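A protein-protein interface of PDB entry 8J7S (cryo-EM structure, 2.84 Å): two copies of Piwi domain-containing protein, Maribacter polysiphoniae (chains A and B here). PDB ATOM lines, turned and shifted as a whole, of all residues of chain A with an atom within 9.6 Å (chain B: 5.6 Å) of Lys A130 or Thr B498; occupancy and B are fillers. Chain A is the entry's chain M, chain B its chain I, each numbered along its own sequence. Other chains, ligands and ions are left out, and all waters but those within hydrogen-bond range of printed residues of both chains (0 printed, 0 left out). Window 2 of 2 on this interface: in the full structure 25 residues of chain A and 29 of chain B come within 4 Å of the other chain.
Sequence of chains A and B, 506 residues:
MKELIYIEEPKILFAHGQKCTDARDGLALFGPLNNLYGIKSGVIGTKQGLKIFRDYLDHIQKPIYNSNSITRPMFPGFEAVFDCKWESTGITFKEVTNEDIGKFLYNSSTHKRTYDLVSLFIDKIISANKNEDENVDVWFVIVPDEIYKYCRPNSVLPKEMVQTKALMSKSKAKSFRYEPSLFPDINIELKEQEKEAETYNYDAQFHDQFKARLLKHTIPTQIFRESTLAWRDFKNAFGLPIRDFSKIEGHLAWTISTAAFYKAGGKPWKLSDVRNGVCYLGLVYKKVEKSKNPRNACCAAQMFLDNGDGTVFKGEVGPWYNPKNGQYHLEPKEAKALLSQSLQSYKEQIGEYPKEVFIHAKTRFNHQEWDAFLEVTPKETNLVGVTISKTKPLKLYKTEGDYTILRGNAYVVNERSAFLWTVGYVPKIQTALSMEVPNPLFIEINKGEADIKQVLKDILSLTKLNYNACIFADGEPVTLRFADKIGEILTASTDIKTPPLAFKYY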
ATOM      1  N   LYS A  94     -19.242  -2.922  -5.753  1.00  0.00           N
ATOM      2  CA  LYS A  94     -20.619  -2.721  -6.204  1.00  0.00           C
ATOM      3  C   LYS A  94     -20.569  -1.833  -7.443  1.00  0.00           C
ATOM      4  O   LYS A  94     -20.391  -0.616  -7.337  1.00  0.00           O
ATOM      5  CB  LYS A  94     -21.482  -2.097  -5.114  1.00  0.00           C
ATOM      6  CG  LYS A  94     -22.370  -3.086  -4.391  1.00  0.00           C
ATOM      7  CD  LYS A  94     -21.537  -4.047  -3.574  1.00  0.00           C
ATOM      8  CE  LYS A  94     -22.395  -5.081  -2.882  1.00  0.00           C
ATOM      9  NZ  LYS A  94     -21.888  -5.345  -1.511  1.00  0.00           N
ATOM     10  N   ILE A 122     -26.080   6.464  -2.271  1.00  0.00           N
ATOM     11  CA  ILE A 122     -26.453   6.037  -0.928  1.00  0.00           C
ATOM     12  C   ILE A 122     -27.458   4.894  -0.969  1.00  0.00           C
ATOM     13  O   ILE A 122     -27.449   4.037  -0.083  1.00  0.00           O
ATOM     14  CB  ILE A 122     -26.953   7.238  -0.096  1.00  0.00           C
ATOM     15  CG1 ILE A 122     -28.357   7.678  -0.517  1.00  0.00           C
ATOM     16  CG2 ILE A 122     -25.955   8.384  -0.146  1.00  0.00           C
ATOM     17  CD1 ILE A 122     -29.448   7.249   0.433  1.00  0.00           C
ATOM     18  N   ASP A 123     -28.326   4.837  -1.984  1.00  0.00           N
ATOM     19  CA  ASP A 123     -29.209   3.682  -2.110  1.00  0.00           C
ATOM     20  C   ASP A 123     -28.420   2.411  -2.381  1.00  0.00           C
ATOM     21  O   ASP A 123     -28.722   1.360  -1.807  1.00  0.00           O
ATOM     22  CB  ASP A 123     -30.250   3.914  -3.204  1.00  0.00           C
ATOM     23  CG  ASP A 123     -31.225   5.021  -2.858  1.00  0.00           C
ATOM     24  OD1 ASP A 123     -31.072   5.633  -1.781  1.00  0.00           O
ATOM     25  OD2 ASP A 123     -32.146   5.277  -3.661  1.00  0.00           O
ATOM     26  N   LYS A 124     -27.402   2.481  -3.245  1.00  0.00           N
ATOM     27  CA  LYS A 124     -26.571   1.302  -3.467  1.00  0.00           C
ATOM     28  C   LYS A 124     -25.855   0.882  -2.188  1.00  0.00           C
ATOM     29  O   LYS A 124     -25.816  -0.309  -1.849  1.00  0.00           O
ATOM     30  CB  LYS A 124     -25.564   1.562  -4.584  1.00  0.00           C
ATOM     31  CG  LYS A 124     -26.013   1.043  -5.936  1.00  0.00           C
ATOM     32  CD  LYS A 124     -24.835   0.594  -6.776  1.00  0.00           C
ATOM     33  CE  LYS A 124     -25.297  -0.207  -7.979  1.00  0.00           C
ATOM     34  NZ  LYS A 124     -26.163   0.600  -8.881  1.00  0.00           N
ATOM     35  N   ILE A 125     -25.298   1.850  -1.455  1.00  0.00           N
ATOM     36  CA  ILE A 125     -24.589   1.522  -0.217  1.00  0.00           C
ATOM     37  C   ILE A 125     -25.537   0.908   0.805  1.00  0.00           C
ATOM     38  O   ILE A 125     -25.201  -0.079   1.466  1.00  0.00           O
ATOM     39  CB  ILE A 125     -23.877   2.764   0.351  1.00  0.00           C
ATOM     40  CG1 ILE A 125     -23.018   3.432  -0.721  1.00  0.00           C
ATOM     41  CG2 ILE A 125     -23.020   2.383   1.544  1.00  0.00           C
ATOM     42  CD1 ILE A 125     -22.141   4.534  -0.189  1.00  0.00           C
ATOM     43  N   ILE A 126     -26.733   1.481   0.955  1.00  0.00           N
ATOM     44  CA  ILE A 126     -27.677   0.986   1.953  1.00  0.00           C
ATOM     45  C   ILE A 126     -28.201  -0.391   1.566  1.00  0.00           C
ATOM     46  O   ILE A 126     -28.390  -1.258   2.427  1.00  0.00           O
ATOM     47  CB  ILE A 126     -28.819   1.998   2.151  1.00  0.00           C
ATOM     48  CG1 ILE A 126     -28.297   3.248   2.854  1.00  0.00           C
ATOM     49  CG2 ILE A 126     -29.946   1.387   2.960  1.00  0.00           C
ATOM     50  CD1 ILE A 126     -29.140   4.465   2.610  1.00  0.00           C
ATOM     51  N   SER A 127     -28.450  -0.618   0.275  1.00  0.00           N
ATOM     52  CA  SER A 127     -28.862  -1.945  -0.167  1.00  0.00           C
ATOM     53  C   SER A 127     -27.777  -2.972   0.125  1.00  0.00           C
ATOM     54  O   SER A 127     -28.057  -4.057   0.645  1.00  0.00           O
ATOM     55  CB  SER A 127     -29.198  -1.921  -1.658  1.00  0.00           C
ATOM     56  OG  SER A 127     -28.044  -2.160  -2.442  1.00  0.00           O
ATOM     57  N   ALA A 128     -26.520  -2.636  -0.182  1.00  0.00           N
ATOM     58  CA  ALA A 128     -25.427  -3.558   0.105  1.00  0.00           C
ATOM     59  C   ALA A 128     -25.252  -3.781   1.601  1.00  0.00           C
ATOM     60  O   ALA A 128     -24.849  -4.870   2.022  1.00  0.00           O
ATOM     61  CB  ALA A 128     -24.132  -3.036  -0.509  1.00  0.00           C
ATOM     62  N   ASN A 129     -25.541  -2.768   2.414  1.00  0.00           N
ATOM     63  CA  ASN A 129     -25.385  -2.897   3.857  1.00  0.00           C
ATOM     64  C   ASN A 129     -26.489  -3.747   4.475  1.00  0.00           C
ATOM     65  O   ASN A 129     -26.225  -4.552   5.374  1.00  0.00           O
ATOM     66  CB  ASN A 129     -25.359  -1.509   4.498  1.00  0.00           C
ATOM     67  CG  ASN A 129     -25.411  -1.564   6.008  1.00  0.00           C
ATOM     68  OD1 ASN A 129     -24.664  -2.310   6.639  1.00  0.00           O
ATOM     69  ND2 ASN A 129     -26.299  -0.775   6.596  1.00  0.00           N
ATOM     70  N   LYS A 130     -27.728  -3.575   4.013  1.00  0.00           N
ATOM     71  CA  LYS A 130     -28.858  -4.256   4.634  1.00  0.00           C
ATOM     72  C   LYS A 130     -28.919  -5.734   4.271  1.00  0.00           C
ATOM     73  O   LYS A 130     -29.177  -6.573   5.139  1.00  0.00           O
ATOM     74  CB  LYS A 130     -30.167  -3.574   4.238  1.00  0.00           C
ATOM     75  CG  LYS A 130     -30.385  -2.222   4.877  1.00  0.00           C
ATOM     76  CD  LYS A 130     -31.643  -1.565   4.340  1.00  0.00           C
ATOM     77  CE  LYS A 130     -32.865  -2.021   5.113  1.00  0.00           C
ATOM     78  NZ  LYS A 130     -32.867  -1.487   6.502  1.00  0.00           N
ATOM     79  N   ASN A 131     -28.693  -6.077   3.006  1.00  0.00           N
ATOM     80  CA  ASN A 131     -29.004  -7.415   2.514  1.00  0.00           C
ATOM     81  C   ASN A 131     -27.850  -7.990   1.705  1.00  0.00           C
ATOM     82  O   ASN A 131     -28.022  -8.480   0.588  1.00  0.00           O
ATOM     83  CB  ASN A 131     -30.293  -7.408   1.699  1.00  0.00           C
ATOM     84  CG  ASN A 131     -30.365  -6.261   0.719  1.00  0.00           C
ATOM     85  OD1 ASN A 131     -29.552  -6.161  -0.198  1.00  0.00           O
ATOM     86  ND2 ASN A 131     -31.348  -5.389   0.902  1.00  0.00           N
ATOM     87  N   GLU A 132     -26.644  -7.925   2.260  1.00  0.00           N
ATOM     88  CA  GLU A 132     -25.524  -8.702   1.757  1.00  0.00           C
ATOM     89  C   GLU A 132     -24.841  -9.393   2.928  1.00  0.00           C
ATOM     90  O   GLU A 132     -24.828  -8.882   4.049  1.00  0.00           O
ATOM     91  CB  GLU A 132     -24.520  -7.842   0.984  1.00  0.00           C
ATOM     92  CG  GLU A 132     -23.559  -8.651   0.124  1.00  0.00           C
ATOM     93  CD  GLU A 132     -22.213  -7.978  -0.048  1.00  0.00           C
ATOM     94  OE1 GLU A 132     -21.756  -7.295   0.892  1.00  0.00           O
ATOM     95  OE2 GLU A 132     -21.611  -8.129  -1.132  1.00  0.00           O
ATOM     96  N   ASP A 133     -24.283 -10.571   2.655  1.00  0.00           N
ATOM     97  CA  ASP A 133     -23.754 -11.404   3.728  1.00  0.00           C
ATOM     98  C   ASP A 133     -22.423 -10.882   4.256  1.00  0.00           C
ATOM     99  O   ASP A 133     -22.088 -11.117   5.423  1.00  0.00           O
ATOM    100  CB  ASP A 133     -23.609 -12.844   3.233  1.00  0.00           C
ATOM    101  CG  ASP A 133     -24.881 -13.655   3.412  1.00  0.00           C
ATOM    102  OD1 ASP A 133     -25.673 -13.342   4.328  1.00  0.00           O
ATOM    103  OD2 ASP A 133     -25.096 -14.600   2.624  1.00  0.00           O
ATOM    104  N   GLU A 134     -21.663 -10.172   3.427  1.00  0.00           N
ATOM    105  CA  GLU A 134     -20.343  -9.698   3.812  1.00  0.00           C
ATOM    106  C   GLU A 134     -20.439  -8.579   4.847  1.00  0.00           C
ATOM    107  O   GLU A 134     -21.453  -7.887   4.968  1.00  0.00           O
ATOM    108  CB  GLU A 134     -19.576  -9.206   2.580  1.00  0.00           C
ATOM    109  CG  GLU A 134     -18.048  -8.973   2.710  1.00  0.00           C
ATOM    110  CD  GLU A 134     -17.288  -9.884   3.680  1.00  0.00           C
ATOM    111  OE1 GLU A 134     -17.763 -10.979   4.041  1.00  0.00           O
ATOM    112  OE2 GLU A 134     -16.183  -9.480   4.095  1.00  0.00           O
ATOM    113  N   VAL A 136     -18.602  -5.128   5.848  1.00  0.00           N
ATOM    114  CA  VAL A 136     -17.730  -4.081   5.328  1.00  0.00           C
ATOM    115  C   VAL A 136     -17.527  -3.038   6.417  1.00  0.00           C
ATOM    116  O   VAL A 136     -18.499  -2.542   7.000  1.00  0.00           O
ATOM    117  CB  VAL A 136     -18.315  -3.443   4.056  1.00  0.00           C
ATOM    118  CG1 VAL A 136     -17.485  -2.253   3.629  1.00  0.00           C
ATOM    119  CG2 VAL A 136     -18.390  -4.468   2.942  1.00  0.00           C
ATOM    120  N   TRP A 139     -16.555   2.066   3.608  1.00  0.00           N
ATOM    121  CA  TRP A 139     -16.970   2.080   2.212  1.00  0.00           C
ATOM    122  C   TRP A 139     -16.217   3.186   1.487  1.00  0.00           C
ATOM    123  O   TRP A 139     -16.318   4.359   1.858  1.00  0.00           O
ATOM    124  CB  TRP A 139     -18.479   2.285   2.087  1.00  0.00           C
ATOM    125  CG  TRP A 139     -19.269   1.037   2.311  1.00  0.00           C
ATOM    126  CD1 TRP A 139     -19.731   0.566   3.500  1.00  0.00           C
ATOM    127  CD2 TRP A 139     -19.685   0.094   1.318  1.00  0.00           C
ATOM    128  NE1 TRP A 139     -20.413  -0.609   3.313  1.00  0.00           N
ATOM    129  CE2 TRP A 139     -20.398  -0.922   1.980  1.00  0.00           C
ATOM    130  CE3 TRP A 139     -19.523   0.009  -0.067  1.00  0.00           C
ATOM    131  CZ2 TRP A 139     -20.946  -2.007   1.307  1.00  0.00           C
ATOM    132  CZ3 TRP A 139     -20.067  -1.071  -0.731  1.00  0.00           C
ATOM    133  CH2 TRP A 139     -20.772  -2.061  -0.045  1.00  0.00           C
ATOM    134  N   LYS A 216     -28.544   8.197   9.609  1.00  0.00           N
ATOM    135  CA  LYS A 216     -29.429   7.285  10.323  1.00  0.00           C
ATOM    136  C   LYS A 216     -28.967   5.838  10.239  1.00  0.00           C
ATOM    137  O   LYS A 216     -29.396   5.015  11.054  1.00  0.00           O
ATOM    138  CB  LYS A 216     -30.856   7.409   9.787  1.00  0.00           C
ATOM    139  CG  LYS A 216     -31.065   6.768   8.424  1.00  0.00           C
ATOM    140  CD  LYS A 216     -32.194   7.439   7.660  1.00  0.00           C
ATOM    141  CE  LYS A 216     -31.884   8.901   7.379  1.00  0.00           C
ATOM    142  NZ  LYS A 216     -30.445   9.125   7.067  1.00  0.00           N
ATOM    143  N   HIS A 217     -28.109   5.508   9.275  1.00  0.00           N
ATOM    144  CA  HIS A 217     -27.599   4.155   9.119  1.00  0.00           C
ATOM    145  C   HIS A 217     -26.219   3.953   9.731  1.00  0.00           C
ATOM    146  O   HIS A 217     -25.865   2.813  10.047  1.00  0.00           O
ATOM    147  CB  HIS A 217     -27.557   3.780   7.636  1.00  0.00           C
ATOM    148  CG  HIS A 217     -28.800   4.144   6.889  1.00  0.00           C
ATOM    149  ND1 HIS A 217     -30.009   3.519   7.104  1.00  0.00           N
ATOM    150  CD2 HIS A 217     -29.026   5.079   5.936  1.00  0.00           C
ATOM    151  CE1 HIS A 217     -30.924   4.046   6.311  1.00  0.00           C
ATOM    152  NE2 HIS A 217     -30.354   4.996   5.593  1.00  0.00           N
ATOM    153  N   ILE A 219     -22.874   4.383   8.584  1.00  0.00           N
ATOM    154  CA  ILE A 219     -21.893   3.663   7.781  1.00  0.00           C
ATOM    155  C   ILE A 219     -20.660   4.553   7.632  1.00  0.00           C
ATOM    156  O   ILE A 219     -20.731   5.596   6.965  1.00  0.00           O
ATOM    157  CB  ILE A 219     -22.456   3.265   6.411  1.00  0.00           C
ATOM    158  CG1 ILE A 219     -23.756   2.476   6.565  1.00  0.00           C
ATOM    159  CG2 ILE A 219     -21.439   2.463   5.635  1.00  0.00           C
ATOM    160  CD1 ILE A 219     -24.837   2.914   5.613  1.00  0.00           C
ATOM    161  N   LEU B 215     -33.660  -3.919  14.167  1.00  0.00           N
ATOM    162  CA  LEU B 215     -33.589  -4.015  12.714  1.00  0.00           C
ATOM    163  C   LEU B 215     -33.471  -2.664  12.024  1.00  0.00           C
ATOM    164  O   LEU B 215     -33.164  -2.626  10.828  1.00  0.00           O
ATOM    165  CB  LEU B 215     -34.817  -4.757  12.183  1.00  0.00           C
ATOM    166  CG  LEU B 215     -34.980  -6.198  12.667  1.00  0.00           C
ATOM    167  CD1 LEU B 215     -36.321  -6.762  12.232  1.00  0.00           C
ATOM    168  CD2 LEU B 215     -33.841  -7.065  12.164  1.00  0.00           C
ATOM    169  N   THR B 218     -29.329  -2.369  11.648  1.00  0.00           N
ATOM    170  CA  THR B 218     -28.520  -3.449  11.078  1.00  0.00           C
ATOM    171  C   THR B 218     -27.319  -3.772  11.969  1.00  0.00           C
ATOM    172  O   THR B 218     -26.160  -3.629  11.579  1.00  0.00           O
ATOM    173  CB  THR B 218     -28.068  -3.119   9.650  1.00  0.00           C
ATOM    174  OG1 THR B 218     -26.965  -2.207   9.695  1.00  0.00           O
ATOM    175  CG2 THR B 218     -29.205  -2.505   8.852  1.00  0.00           C
ATOM    176  N   ILE B 496     -42.486  -1.859  11.210  1.00  0.00           N
ATOM    177  CA  ILE B 496     -41.232  -2.141  10.516  1.00  0.00           C
ATOM    178  C   ILE B 496     -41.428  -1.849   9.036  1.00  0.00           C
ATOM    179  O   ILE B 496     -42.368  -2.354   8.414  1.00  0.00           O
ATOM    180  CB  ILE B 496     -40.768  -3.597  10.731  1.00  0.00           C
ATOM    181  CG1 ILE B 496     -39.970  -3.725  12.029  1.00  0.00           C
ATOM    182  CG2 ILE B 496     -39.925  -4.074   9.560  1.00  0.00           C
ATOM    183  CD1 ILE B 496     -39.926  -5.128  12.583  1.00  0.00           C
ATOM    184  N   LYS B 497     -40.548  -1.026   8.475  1.00  0.00           N
ATOM    185  CA  LYS B 497     -40.545  -0.725   7.050  1.00  0.00           C
ATOM    186  C   LYS B 497     -39.200  -1.126   6.468  1.00  0.00           C
ATOM    187  O   LYS B 497     -38.152  -0.767   7.016  1.00  0.00           O
ATOM    188  CB  LYS B 497     -40.815   0.759   6.792  1.00  0.00           C
ATOM    189  CG  LYS B 497     -41.519   1.472   7.932  1.00  0.00           C
ATOM    190  CD  LYS B 497     -43.019   1.234   7.885  1.00  0.00           C
ATOM    191  CE  LYS B 497     -43.736   2.029   8.962  1.00  0.00           C
ATOM    192  NZ  LYS B 497     -45.191   2.164   8.676  1.00  0.00           N
ATOM    193  N   THR B 498     -39.236  -1.866   5.358  1.00  0.00           N
ATOM    194  CA  THR B 498     -38.046  -2.355   4.668  1.00  0.00           C
ATOM    195  C   THR B 498     -37.122  -3.095   5.627  1.00  0.00           C
ATOM    196  O   THR B 498     -36.078  -2.558   6.020  1.00  0.00           O
ATOM    197  CB  THR B 498     -37.295  -1.202   3.998  1.00  0.00           C
ATOM    198  OG1 THR B 498     -38.223  -0.180   3.619  1.00  0.00           O
ATOM    199  CG2 THR B 498     -36.560  -1.696   2.762  1.00  0.00           C
ATOM    200  N   PRO B 499     -37.469  -4.312   6.034  1.00  0.00           N
ATOM    201  CA  PRO B 499     -36.590  -5.081   6.919  1.00  0.00           C
ATOM    202  C   PRO B 499     -35.261  -5.367   6.243  1.00  0.00           C
ATOM    203  O   PRO B 499     -35.177  -5.387   5.005  1.00  0.00           O
ATOM    204  CB  PRO B 499     -37.382  -6.371   7.176  1.00  0.00           C
ATOM    205  CG  PRO B 499     -38.337  -6.466   6.038  1.00  0.00           C
ATOM    206  CD  PRO B 499     -38.685  -5.059   5.672  1.00  0.00           C
ATOM    207  N   PRO B 500     -34.196  -5.572   7.023  1.00  0.00           N
ATOM    208  CA  PRO B 500     -32.852  -5.658   6.427  1.00  0.00           C
ATOM    209  C   PRO B 500     -32.693  -6.754   5.386  1.00  0.00           C
ATOM    210  O   PRO B 500     -31.901  -6.580   4.451  1.00  0.00           O
ATOM    211  CB  PRO B 500     -31.948  -5.898   7.643  1.00  0.00           C
ATOM    212  CG  PRO B 500     -32.866  -6.241   8.775  1.00  0.00           C
ATOM    213  CD  PRO B 500     -34.147  -5.553   8.491  1.00  0.00           C
ATOM    214  N   LEU B 501     -33.389  -7.881   5.531  1.00  0.00           N
ATOM    215  CA  LEU B 501     -33.538  -8.933   4.516  1.00  0.00           C
ATOM    216  C   LEU B 501     -32.309  -9.835   4.423  1.00  0.00           C
ATOM    217  O   LEU B 501     -32.274 -10.730   3.575  1.00  0.00           O
ATOM    218  CB  LEU B 501     -33.899  -8.311   3.156  1.00  0.00           C
ATOM    219  CG  LEU B 501     -34.249  -9.006   1.834  1.00  0.00           C
ATOM    220  CD1 LEU B 501     -35.106  -8.069   1.009  1.00  0.00           C
ATOM    221  CD2 LEU B 501     -33.038  -9.391   1.011  1.00  0.00           C
ATOM    222  N   ALA B 502     -31.322  -9.672   5.302  1.00  0.00           N
ATOM    223  CA  ALA B 502     -30.176 -10.569   5.376  1.00  0.00           C
ATOM    224  C   ALA B 502     -30.228 -11.356   6.678  1.00  0.00           C
ATOM    225  O   ALA B 502     -30.627 -10.833   7.720  1.00  0.00           O
ATOM    226  CB  ALA B 502     -28.854  -9.808   5.282  1.00  0.00           C
ATOM    227  N   LYS B 504     -28.138 -12.585   8.855  1.00  0.00           N
ATOM    228  CA  LYS B 504     -27.295 -12.399  10.033  1.00  0.00           C
ATOM    229  C   LYS B 504     -27.998 -11.581  11.107  1.00  0.00           C
ATOM    230  O   LYS B 504     -27.730 -11.765  12.298  1.00  0.00           O
ATOM    231  CB  LYS B 504     -25.972 -11.739   9.648  1.00  0.00           C
ATOM    232  CG  LYS B 504     -26.104 -10.553   8.711  1.00  0.00           C
ATOM    233  CD  LYS B 504     -24.739 -10.002   8.341  1.00  0.00           C
ATOM    234  CE  LYS B 504     -24.843  -8.975   7.231  1.00  0.00           C
ATOM    235  NZ  LYS B 504     -23.583  -8.205   7.064  1.00  0.00           N
ATOM    236  N   TYR B 505     -28.896 -10.684  10.711  1.00  0.00           N
ATOM    237  CA  TYR B 505     -29.632  -9.870  11.668  1.00  0.00           C
ATOM    238  C   TYR B 505     -30.772 -10.622  12.338  1.00  0.00           C
ATOM    239  O   TYR B 505     -31.365 -10.096  13.285  1.00  0.00           O
ATOM    240  CB  TYR B 505     -30.177  -8.626  10.974  1.00  0.00           C
ATOM    241  CG  TYR B 505     -29.149  -7.903  10.141  1.00  0.00           C
ATOM    242  CD1 TYR B 505     -27.956  -7.466  10.694  1.00  0.00           C
ATOM    243  CD2 TYR B 505     -29.368  -7.671   8.794  1.00  0.00           C
ATOM    244  CE1 TYR B 505     -27.016  -6.806   9.931  1.00  0.00           C
ATOM    245  CE2 TYR B 505     -28.437  -7.013   8.022  1.00  0.00           C
ATOM    246  CZ  TYR B 505     -27.264  -6.582   8.593  1.00  0.00           C
ATOM    247  OH  TYR B 505     -26.336  -5.929   7.818  1.00  0.00           O
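OG1 of Thr B218 lies within hydrogen-bond range of ND2 of Asn A129 (3.5 Å).
The backbone carbonyl oxygen (O) of Thr B498 lies close to the side-chain amino group (NZ) of Lys A130, 3.4 Å away.
The side-chain amino group (NZ) of Lys B504 sits close to the backbone carbonyl oxygen (O) of Glu A132 (3.3 Å).
The side-chain amino group (NZ) of Lys B504 lies within hydrogen-bond range of the backbone carbonyl oxygen (O) of Glu A134 (3.0 Å).
The side-chain hydroxyl (OH) of Tyr B505 is in hydrogen-bond range of the backbone carbonyl oxygen (O) of Asn A129.
O of Pro B500 sits close to O of Lys A130.
The side-chain carboxylate (OE2) of Glu A132 is in salt-bridge range of the side-chain amino group (NZ) of Lys A94, at 2.8 Å.
The backbone carbonyl oxygen of Ser A127 sits close to the side-chain amide oxygen of Asn A131, 2.7 Å away.
Among the printed residues, pairs that only touch across the chains: Lys A130 with Ala B502 (3.3 Å), Lys A130 with Tyr B505 (3.0 Å), Asn A131 with Pro B500 (3.3 Å), Asn A131 with Leu B501 (3.5 Å), Asn A131 with Ala B502 (3.7 Å) and Asp A133 with Lys B504 (3.7 Å).
Lys A130 touches just these residues of chain B: Thr B498, Pro B500, Ala B502 and Tyr B505.
Thr B498 touches just one residue of chain A: Lys A130 (3.4 Å).
Of the printed residues of chain A, Tyr B505 touches Asn A129 (2.8 Å) and Lys A130 (3.0 Å).
Printed residues of chain B within 4 Å of Glu A134: Lys B504.
The nearest residue of chain A that does not touch Thr B498 is Asn A131 (6.7 Å).
Along chain B the printed residues that touch a printed residue of chain A span positions 218 to 505.
Among the printed residues, 12 pairs touch across the chains.
No position is printed for both chains.
Of the 12 pairs that touch across the chains among the printed residues, none has its exchanged pair printed and touching as well.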
